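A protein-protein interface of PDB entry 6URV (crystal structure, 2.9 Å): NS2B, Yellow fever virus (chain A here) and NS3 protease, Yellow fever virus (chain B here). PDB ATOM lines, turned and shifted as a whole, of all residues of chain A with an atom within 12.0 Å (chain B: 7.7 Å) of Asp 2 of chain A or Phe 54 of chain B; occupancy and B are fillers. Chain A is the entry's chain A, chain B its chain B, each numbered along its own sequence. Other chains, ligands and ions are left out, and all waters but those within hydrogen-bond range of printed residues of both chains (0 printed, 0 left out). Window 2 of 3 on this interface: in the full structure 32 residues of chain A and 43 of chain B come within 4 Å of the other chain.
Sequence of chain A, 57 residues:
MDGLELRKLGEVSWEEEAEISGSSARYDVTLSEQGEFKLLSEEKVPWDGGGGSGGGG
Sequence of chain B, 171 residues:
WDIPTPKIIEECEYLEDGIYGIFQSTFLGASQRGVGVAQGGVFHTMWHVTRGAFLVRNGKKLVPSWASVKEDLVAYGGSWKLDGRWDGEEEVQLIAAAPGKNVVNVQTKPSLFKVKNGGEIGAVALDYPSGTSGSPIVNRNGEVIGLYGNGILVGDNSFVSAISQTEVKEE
O of Leu 55 of chain B sits at hydrogen-bond distance from N of Leu 62 of chain B, at 2.9 Å.
OE2 of Glu 5 of chain A is in salt-bridge range of NE of Arg 7 of chain A, 3.3 Å away.
N of Val 56 of chain B lies within hydrogen-bond range of O of Leu 4 of chain A (2.9 Å).
O of Val 56 of chain B sits at hydrogen-bond distance from N of Leu 6 of chain A (3.3 Å).
The backbone carbonyl oxygen (O) of Phe 54 of chain B lies within hydrogen-bond range of the backbone NH (N) of Leu 4 of chain A.
N of Glu 5 of chain A sits at hydrogen-bond distance from O of Phe 23 of chain B, at 3.0 Å.
Of the 17 printed residues of chain B, 6 touch a printed residue of chain A.
Hydrophobic or aromatic side chains of chain B that line the printed part of chain A: Ile 22, Phe 23, Phe 54, Leu 55 and Val 56.
Of the 7 printed residues of chain A, 6 touch a printed residue of chain B.
Printed residues of chain A that touch a printed residue of chain B: Asp 2, Gly 3, Leu 4, Glu 5, Leu 6 and Arg 7.
Hydrophobic or aromatic side chains of chain A within 4 Å of the printed part of chain B: Leu 4 and Leu 6.
Among the printed residues, 15 pairs touch across the chains.
Among the printed residues, no Asp or Glu carboxylate lies within 4 Å of a Lys or Arg side-chain nitrogen of the other chain.
Phe 54 of chain B touches just these residues of chain A: Asp 2 (3.7 Å), Gly 3 (3.6 Å) and Leu 4 (3.3 Å).
No residue of chain A comes within 4 Å of Ser 25 of chain B.
Of chain A, only Leu 4 (3.2 Å) and Leu 6 (3.7 Å) come within 4 Å of Leu 55 of chain B.
No residue of chain A comes within 4 Å of Lys 61 of chain B.
No residue of chain A comes within 4 Å of Val 63 of chain B.
Of the printed residues of chain B, Gly 3 of chain A touches Phe 54.
Printed residues of chain A within 4 Å of Gln 24 of chain B: Leu 4.
Printed residues of chain A within 4 Å of Phe 23 of chain B: Leu 4 (3.2 Å), Glu 5 (3.0 Å) and Arg 7 (3.4 Å).
Of the printed residues of chain B, Glu 5 of chain A touches Ile 22 (3.8 Å), Phe 23 (3.0 Å) and Val 56 (3.6 Å).
The nearest printed residue of chain B that does not touch Arg 7 of chain A is Ile 22 of chain B (5.4 Å).
O of Asp 2 of chain A touches CZ of Phe 54 of chain B, 3.7 Å away.
Gly 3 of chain A touches Phe 54 of chain B (CA to CE1, 3.6 Å).
CD1 of Leu 4 of chain A touches CG2 of Ile 22 of chain B, 3.6 Å away.
Leu 4 of chain A touches Phe 23 of chain B.
Gln 24 of chain B touches Leu 4 of chain A (CB to CD2, 3.6 Å).
O of Leu 4 of chain A touches CA of Leu 55 of chain B, 3.2 Å away.
Glu 5 of chain A touches Ile 22 of chain B (O to CA, 3.8 Å).
Glu 5 of chain A touches Val 56 of chain B.
CD2 of Leu 6 of chain A touches CG of Leu 55 of chain B, at 3.7 Å.
Arg 7 of chain A touches Phe 23 of chain B.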
ATOM      1  N   MET A   1      24.754  17.125  32.823  1.00  0.00           N
ATOM      2  CA  MET A   1      23.430  17.695  33.054  1.00  0.00           C
ATOM      3  C   MET A   1      23.364  19.137  32.558  1.00  0.00           C
ATOM      4  O   MET A   1      22.448  19.885  32.905  1.00  0.00           O
ATOM      5  CB  MET A   1      23.068  17.626  34.539  1.00  0.00           C
ATOM      6  N   ASP A   2      24.346  19.517  31.742  1.00  0.00           N
ATOM      7  CA  ASP A   2      24.421  20.855  31.166  1.00  0.00           C
ATOM      8  C   ASP A   2      23.936  20.912  29.726  1.00  0.00           C
ATOM      9  O   ASP A   2      23.566  21.992  29.253  1.00  0.00           O
ATOM     10  CB  ASP A   2      25.858  21.384  31.237  1.00  0.00           C
ATOM     11  CG  ASP A   2      26.339  21.555  32.664  1.00  0.00           C
ATOM     12  OD1 ASP A   2      25.533  21.997  33.513  1.00  0.00           O
ATOM     13  OD2 ASP A   2      27.517  21.246  32.942  1.00  0.00           O
ATOM     14  N   GLY A   3      23.939  19.788  29.021  1.00  0.00           N
ATOM     15  CA  GLY A   3      23.477  19.750  27.652  1.00  0.00           C
ATOM     16  C   GLY A   3      22.650  18.511  27.393  1.00  0.00           C
ATOM     17  O   GLY A   3      22.323  17.768  28.324  1.00  0.00           O
ATOM     18  N   LEU A   4      22.294  18.281  26.138  1.00  0.00           N
ATOM     19  CA  LEU A   4      21.489  17.132  25.770  1.00  0.00           C
ATOM     20  C   LEU A   4      22.355  16.135  25.016  1.00  0.00           C
ATOM     21  O   LEU A   4      23.277  16.514  24.289  1.00  0.00           O
ATOM     22  CB  LEU A   4      20.298  17.559  24.912  1.00  0.00           C
ATOM     23  CG  LEU A   4      19.748  18.934  25.299  1.00  0.00           C
ATOM     24  CD1 LEU A   4      18.889  19.518  24.192  1.00  0.00           C
ATOM     25  CD2 LEU A   4      18.973  18.861  26.609  1.00  0.00           C
ATOM     26  N   GLU A   5      22.048  14.855  25.191  1.00  0.00           N
ATOM     27  CA  GLU A   5      22.852  13.780  24.635  1.00  0.00           C
ATOM     28  C   GLU A   5      22.074  13.130  23.502  1.00  0.00           C
ATOM     29  O   GLU A   5      20.843  13.051  23.536  1.00  0.00           O
ATOM     30  CB  GLU A   5      23.233  12.730  25.698  1.00  0.00           C
ATOM     31  CG  GLU A   5      23.351  11.298  25.160  1.00  0.00           C
ATOM     32  CD  GLU A   5      23.501  10.238  26.239  1.00  0.00           C
ATOM     33  OE1 GLU A   5      24.402  10.382  27.094  1.00  0.00           O
ATOM     34  OE2 GLU A   5      22.729   9.256  26.228  1.00  0.00           O
ATOM     35  N   LEU A   6      22.804  12.648  22.505  1.00  0.00           N
ATOM     36  CA  LEU A   6      22.191  12.059  21.328  1.00  0.00           C
ATOM     37  C   LEU A   6      22.295  10.545  21.395  1.00  0.00           C
ATOM     38  O   LEU A   6      23.312   9.994  21.825  1.00  0.00           O
ATOM     39  CB  LEU A   6      22.880  12.544  20.052  1.00  0.00           C
ATOM     40  CG  LEU A   6      22.984  14.047  19.801  1.00  0.00           C
ATOM     41  CD1 LEU A   6      23.369  14.314  18.357  1.00  0.00           C
ATOM     42  CD2 LEU A   6      21.677  14.738  20.142  1.00  0.00           C
ATOM     43  N   ARG A   7      21.239   9.879  20.951  1.00  0.00           N
ATOM     44  CA  ARG A   7      21.200   8.430  20.885  1.00  0.00           C
ATOM     45  C   ARG A   7      20.594   8.046  19.552  1.00  0.00           C
ATOM     46  O   ARG A   7      19.565   8.592  19.147  1.00  0.00           O
ATOM     47  CB  ARG A   7      20.366   7.814  22.016  1.00  0.00           C
ATOM     48  CG  ARG A   7      20.998   7.865  23.397  1.00  0.00           C
ATOM     49  CD  ARG A   7      20.248   6.942  24.352  1.00  0.00           C
ATOM     50  NE  ARG A   7      19.933   7.590  25.621  1.00  0.00           N
ATOM     51  CZ  ARG A   7      19.083   7.099  26.518  1.00  0.00           C
ATOM     52  NH1 ARG A   7      18.461   5.951  26.283  1.00  0.00           N
ATOM     53  NH2 ARG A   7      18.855   7.755  27.648  1.00  0.00           N
ATOM     54  N   ILE B  22      17.033  13.192  21.058  1.00  0.00           N
ATOM     55  CA  ILE B  22      17.537  14.212  21.964  1.00  0.00           C
ATOM     56  C   ILE B  22      17.070  13.879  23.369  1.00  0.00           C
ATOM     57  O   ILE B  22      15.864  13.756  23.618  1.00  0.00           O
ATOM     58  CB  ILE B  22      17.064  15.622  21.571  1.00  0.00           C
ATOM     59  CG1 ILE B  22      17.396  15.947  20.101  1.00  0.00           C
ATOM     60  CG2 ILE B  22      17.640  16.632  22.537  1.00  0.00           C
ATOM     61  CD1 ILE B  22      18.683  16.668  19.902  1.00  0.00           C
ATOM     62  N   PHE B  23      18.017  13.746  24.291  1.00  0.00           N
ATOM     63  CA  PHE B  23      17.733  13.348  25.662  1.00  0.00           C
ATOM     64  C   PHE B  23      18.222  14.426  26.610  1.00  0.00           C
ATOM     65  O   PHE B  23      19.360  14.883  26.489  1.00  0.00           O
ATOM     66  CB  PHE B  23      18.391  12.005  25.996  1.00  0.00           C
ATOM     67  CG  PHE B  23      17.709  10.838  25.351  1.00  0.00           C
ATOM     68  CD1 PHE B  23      17.921  10.537  24.014  1.00  0.00           C
ATOM     69  CD2 PHE B  23      16.835  10.054  26.081  1.00  0.00           C
ATOM     70  CE1 PHE B  23      17.281   9.467  23.426  1.00  0.00           C
ATOM     71  CE2 PHE B  23      16.191   8.985  25.501  1.00  0.00           C
ATOM     72  CZ  PHE B  23      16.416   8.691  24.168  1.00  0.00           C
ATOM     73  N   GLN B  24      17.372  14.816  27.557  1.00  0.00           N
ATOM     74  CA  GLN B  24      17.714  15.800  28.573  1.00  0.00           C
ATOM     75  C   GLN B  24      17.774  15.104  29.924  1.00  0.00           C
ATOM     76  O   GLN B  24      16.919  14.270  30.243  1.00  0.00           O
ATOM     77  CB  GLN B  24      16.688  16.944  28.610  1.00  0.00           C
ATOM     78  CG  GLN B  24      16.889  17.937  29.763  1.00  0.00           C
ATOM     79  CD  GLN B  24      15.927  19.119  29.722  1.00  0.00           C
ATOM     80  OE1 GLN B  24      16.279  20.227  30.123  1.00  0.00           O
ATOM     81  NE2 GLN B  24      14.707  18.883  29.244  1.00  0.00           N
ATOM     82  N   SER B  25      18.768  15.464  30.726  1.00  0.00           N
ATOM     83  CA  SER B  25      19.018  14.807  31.999  1.00  0.00           C
ATOM     84  C   SER B  25      18.626  15.755  33.119  1.00  0.00           C
ATOM     85  O   SER B  25      19.164  16.863  33.218  1.00  0.00           O
ATOM     86  CB  SER B  25      20.481  14.389  32.127  1.00  0.00           C
ATOM     87  OG  SER B  25      20.620  13.334  33.066  1.00  0.00           O
ATOM     88  N   THR B  50      15.446  22.282  20.779  1.00  0.00           N
ATOM     89  CA  THR B  50      16.693  22.623  21.455  1.00  0.00           C
ATOM     90  C   THR B  50      16.809  24.096  21.824  1.00  0.00           C
ATOM     91  O   THR B  50      17.465  24.419  22.816  1.00  0.00           O
ATOM     92  CB  THR B  50      17.905  22.236  20.598  1.00  0.00           C
ATOM     93  OG1 THR B  50      18.026  23.139  19.489  1.00  0.00           O
ATOM     94  CG2 THR B  50      17.766  20.806  20.085  1.00  0.00           C
ATOM     95  N   ARG B  51      16.217  24.986  21.026  1.00  0.00           N
ATOM     96  CA  ARG B  51      16.393  26.435  21.164  1.00  0.00           C
ATOM     97  C   ARG B  51      17.872  26.804  21.290  1.00  0.00           C
ATOM     98  O   ARG B  51      18.255  27.682  22.064  1.00  0.00           O
ATOM     99  CB  ARG B  51      15.577  26.977  22.342  1.00  0.00           C
ATOM    100  CG  ARG B  51      14.394  27.850  21.910  1.00  0.00           C
ATOM    101  CD  ARG B  51      13.597  28.403  23.091  1.00  0.00           C
ATOM    102  NE  ARG B  51      12.943  27.354  23.868  1.00  0.00           N
ATOM    103  CZ  ARG B  51      11.731  26.874  23.604  1.00  0.00           C
ATOM    104  NH1 ARG B  51      11.037  27.349  22.578  1.00  0.00           N
ATOM    105  NH2 ARG B  51      11.212  25.920  24.366  1.00  0.00           N
ATOM    106  N   GLY B  52      18.706  26.137  20.490  1.00  0.00           N
ATOM    107  CA  GLY B  52      20.127  26.418  20.415  1.00  0.00           C
ATOM    108  C   GLY B  52      20.998  25.813  21.497  1.00  0.00           C
ATOM    109  O   GLY B  52      22.187  26.141  21.555  1.00  0.00           O
ATOM    110  N   ALA B  53      20.462  24.937  22.348  1.00  0.00           N
ATOM    111  CA  ALA B  53      21.287  24.277  23.354  1.00  0.00           C
ATOM    112  C   ALA B  53      22.259  23.303  22.690  1.00  0.00           C
ATOM    113  O   ALA B  53      21.971  22.725  21.638  1.00  0.00           O
ATOM    114  CB  ALA B  53      20.409  23.539  24.364  1.00  0.00           C
ATOM    115  N   PHE B  54      23.427  23.120  23.311  1.00  0.00           N
ATOM    116  CA  PHE B  54      24.444  22.263  22.715  1.00  0.00           C
ATOM    117  C   PHE B  54      24.189  20.782  22.998  1.00  0.00           C
ATOM    118  O   PHE B  54      23.589  20.411  24.011  1.00  0.00           O
ATOM    119  CB  PHE B  54      25.852  22.688  23.166  1.00  0.00           C
ATOM    120  CG  PHE B  54      26.134  22.534  24.639  1.00  0.00           C
ATOM    121  CD1 PHE B  54      26.343  21.284  25.202  1.00  0.00           C
ATOM    122  CD2 PHE B  54      26.276  23.651  25.443  1.00  0.00           C
ATOM    123  CE1 PHE B  54      26.631  21.152  26.547  1.00  0.00           C
ATOM    124  CE2 PHE B  54      26.568  23.524  26.789  1.00  0.00           C
ATOM    125  CZ  PHE B  54      26.746  22.272  27.341  1.00  0.00           C
ATOM    126  N   LEU B  55      24.645  19.941  22.069  1.00  0.00           N
ATOM    127  CA  LEU B  55      24.559  18.489  22.155  1.00  0.00           C
ATOM    128  C   LEU B  55      25.891  17.891  22.587  1.00  0.00           C
ATOM    129  O   LEU B  55      26.928  18.559  22.607  1.00  0.00           O
ATOM    130  CB  LEU B  55      24.169  17.857  20.815  1.00  0.00           C
ATOM    131  CG  LEU B  55      22.919  18.183  20.007  1.00  0.00           C
ATOM    132  CD1 LEU B  55      21.673  18.369  20.869  1.00  0.00           C
ATOM    133  CD2 LEU B  55      23.199  19.380  19.157  1.00  0.00           C
ATOM    134  N   VAL B  56      25.856  16.602  22.912  1.00  0.00           N
ATOM    135  CA  VAL B  56      27.070  15.852  23.198  1.00  0.00           C
ATOM    136  C   VAL B  56      26.964  14.492  22.528  1.00  0.00           C
ATOM    137  O   VAL B  56      25.929  13.824  22.598  1.00  0.00           O
ATOM    138  CB  VAL B  56      27.338  15.707  24.709  1.00  0.00           C
ATOM    139  CG1 VAL B  56      27.745  17.041  25.300  1.00  0.00           C
ATOM    140  CG2 VAL B  56      26.113  15.157  25.428  1.00  0.00           C
ATOM    141  N   LYS B  60      31.809  14.467  22.574  1.00  0.00           N
ATOM    142  CA  LYS B  60      31.993  15.513  21.572  1.00  0.00           C
ATOM    143  C   LYS B  60      30.824  16.486  21.666  1.00  0.00           C
ATOM    144  O   LYS B  60      29.665  16.081  21.525  1.00  0.00           O
ATOM    145  CB  LYS B  60      32.102  14.934  20.162  1.00  0.00           C
ATOM    146  N   LYS B  61      31.129  17.763  21.873  1.00  0.00           N
ATOM    147  CA  LYS B  61      30.123  18.795  22.088  1.00  0.00           C
ATOM    148  C   LYS B  61      29.816  19.506  20.773  1.00  0.00           C
ATOM    149  O   LYS B  61      30.724  20.021  20.114  1.00  0.00           O
ATOM    150  CB  LYS B  61      30.597  19.800  23.141  1.00  0.00           C
ATOM    151  N   LEU B  62      28.536  19.544  20.407  1.00  0.00           N
ATOM    152  CA  LEU B  62      28.067  20.169  19.177  1.00  0.00           C
ATOM    153  C   LEU B  62      27.360  21.475  19.509  1.00  0.00           C
ATOM    154  O   LEU B  62      26.520  21.515  20.414  1.00  0.00           O
ATOM    155  CB  LEU B  62      27.089  19.251  18.443  1.00  0.00           C
ATOM    156  CG  LEU B  62      27.522  17.917  17.839  1.00  0.00           C
ATOM    157  CD1 LEU B  62      26.436  16.888  18.089  1.00  0.00           C
ATOM    158  CD2 LEU B  62      27.757  18.077  16.352  1.00  0.00           C
ATOM    159  N   VAL B  63      27.683  22.532  18.770  1.00  0.00           N
ATOM    160  CA  VAL B  63      27.039  23.829  18.985  1.00  0.00           C
ATOM    161  C   VAL B  63      26.268  24.215  17.731  1.00  0.00           C
ATOM    162  O   VAL B  63      26.642  23.795  16.626  1.00  0.00           O
ATOM    163  CB  VAL B  63      28.063  24.915  19.351  1.00  0.00           C
ATOM    164  CG1 VAL B  63      28.563  24.714  20.768  1.00  0.00           C
ATOM    165  CG2 VAL B  63      29.209  24.904  18.351  1.00  0.00           C
ATOM    166  N   PRO B  64      25.190  24.994  17.845  1.00  0.00           N
ATOM    167  CA  PRO B  64      24.375  25.300  16.661  1.00  0.00           C
ATOM    168  C   PRO B  64      25.162  26.136  15.669  1.00  0.00           C
ATOM    169  O   PRO B  64      25.795  27.126  16.037  1.00  0.00           O
ATOM    170  CB  PRO B  64      23.180  26.069  17.238  1.00  0.00           C
ATOM    171  CG  PRO B  64      23.645  26.577  18.552  1.00  0.00           C
ATOM    172  CD  PRO B  64      24.613  25.565  19.075  1.00  0.00           C
ATOM    173  N   TYR B  76      23.470  21.794  13.426  1.00  0.00           N
ATOM    174  CA  TYR B  76      24.660  21.729  14.265  1.00  0.00           C
ATOM    175  C   TYR B  76      25.828  21.169  13.466  1.00  0.00           C
ATOM    176  O   TYR B  76      25.706  20.101  12.856  1.00  0.00           O
ATOM    177  CB  TYR B  76      24.414  20.854  15.494  1.00  0.00           C
ATOM    178  CG  TYR B  76      23.442  21.422  16.504  1.00  0.00           C
ATOM    179  CD1 TYR B  76      22.073  21.235  16.370  1.00  0.00           C
ATOM    180  CD2 TYR B  76      23.897  22.123  17.608  1.00  0.00           C
ATOM    181  CE1 TYR B  76      21.188  21.744  17.306  1.00  0.00           C
ATOM    182  CE2 TYR B  76      23.022  22.631  18.545  1.00  0.00           C
ATOM    183  CZ  TYR B  76      21.674  22.440  18.391  1.00  0.00           C
ATOM    184  OH  TYR B  76      20.812  22.952  19.332  1.00  0.00           O
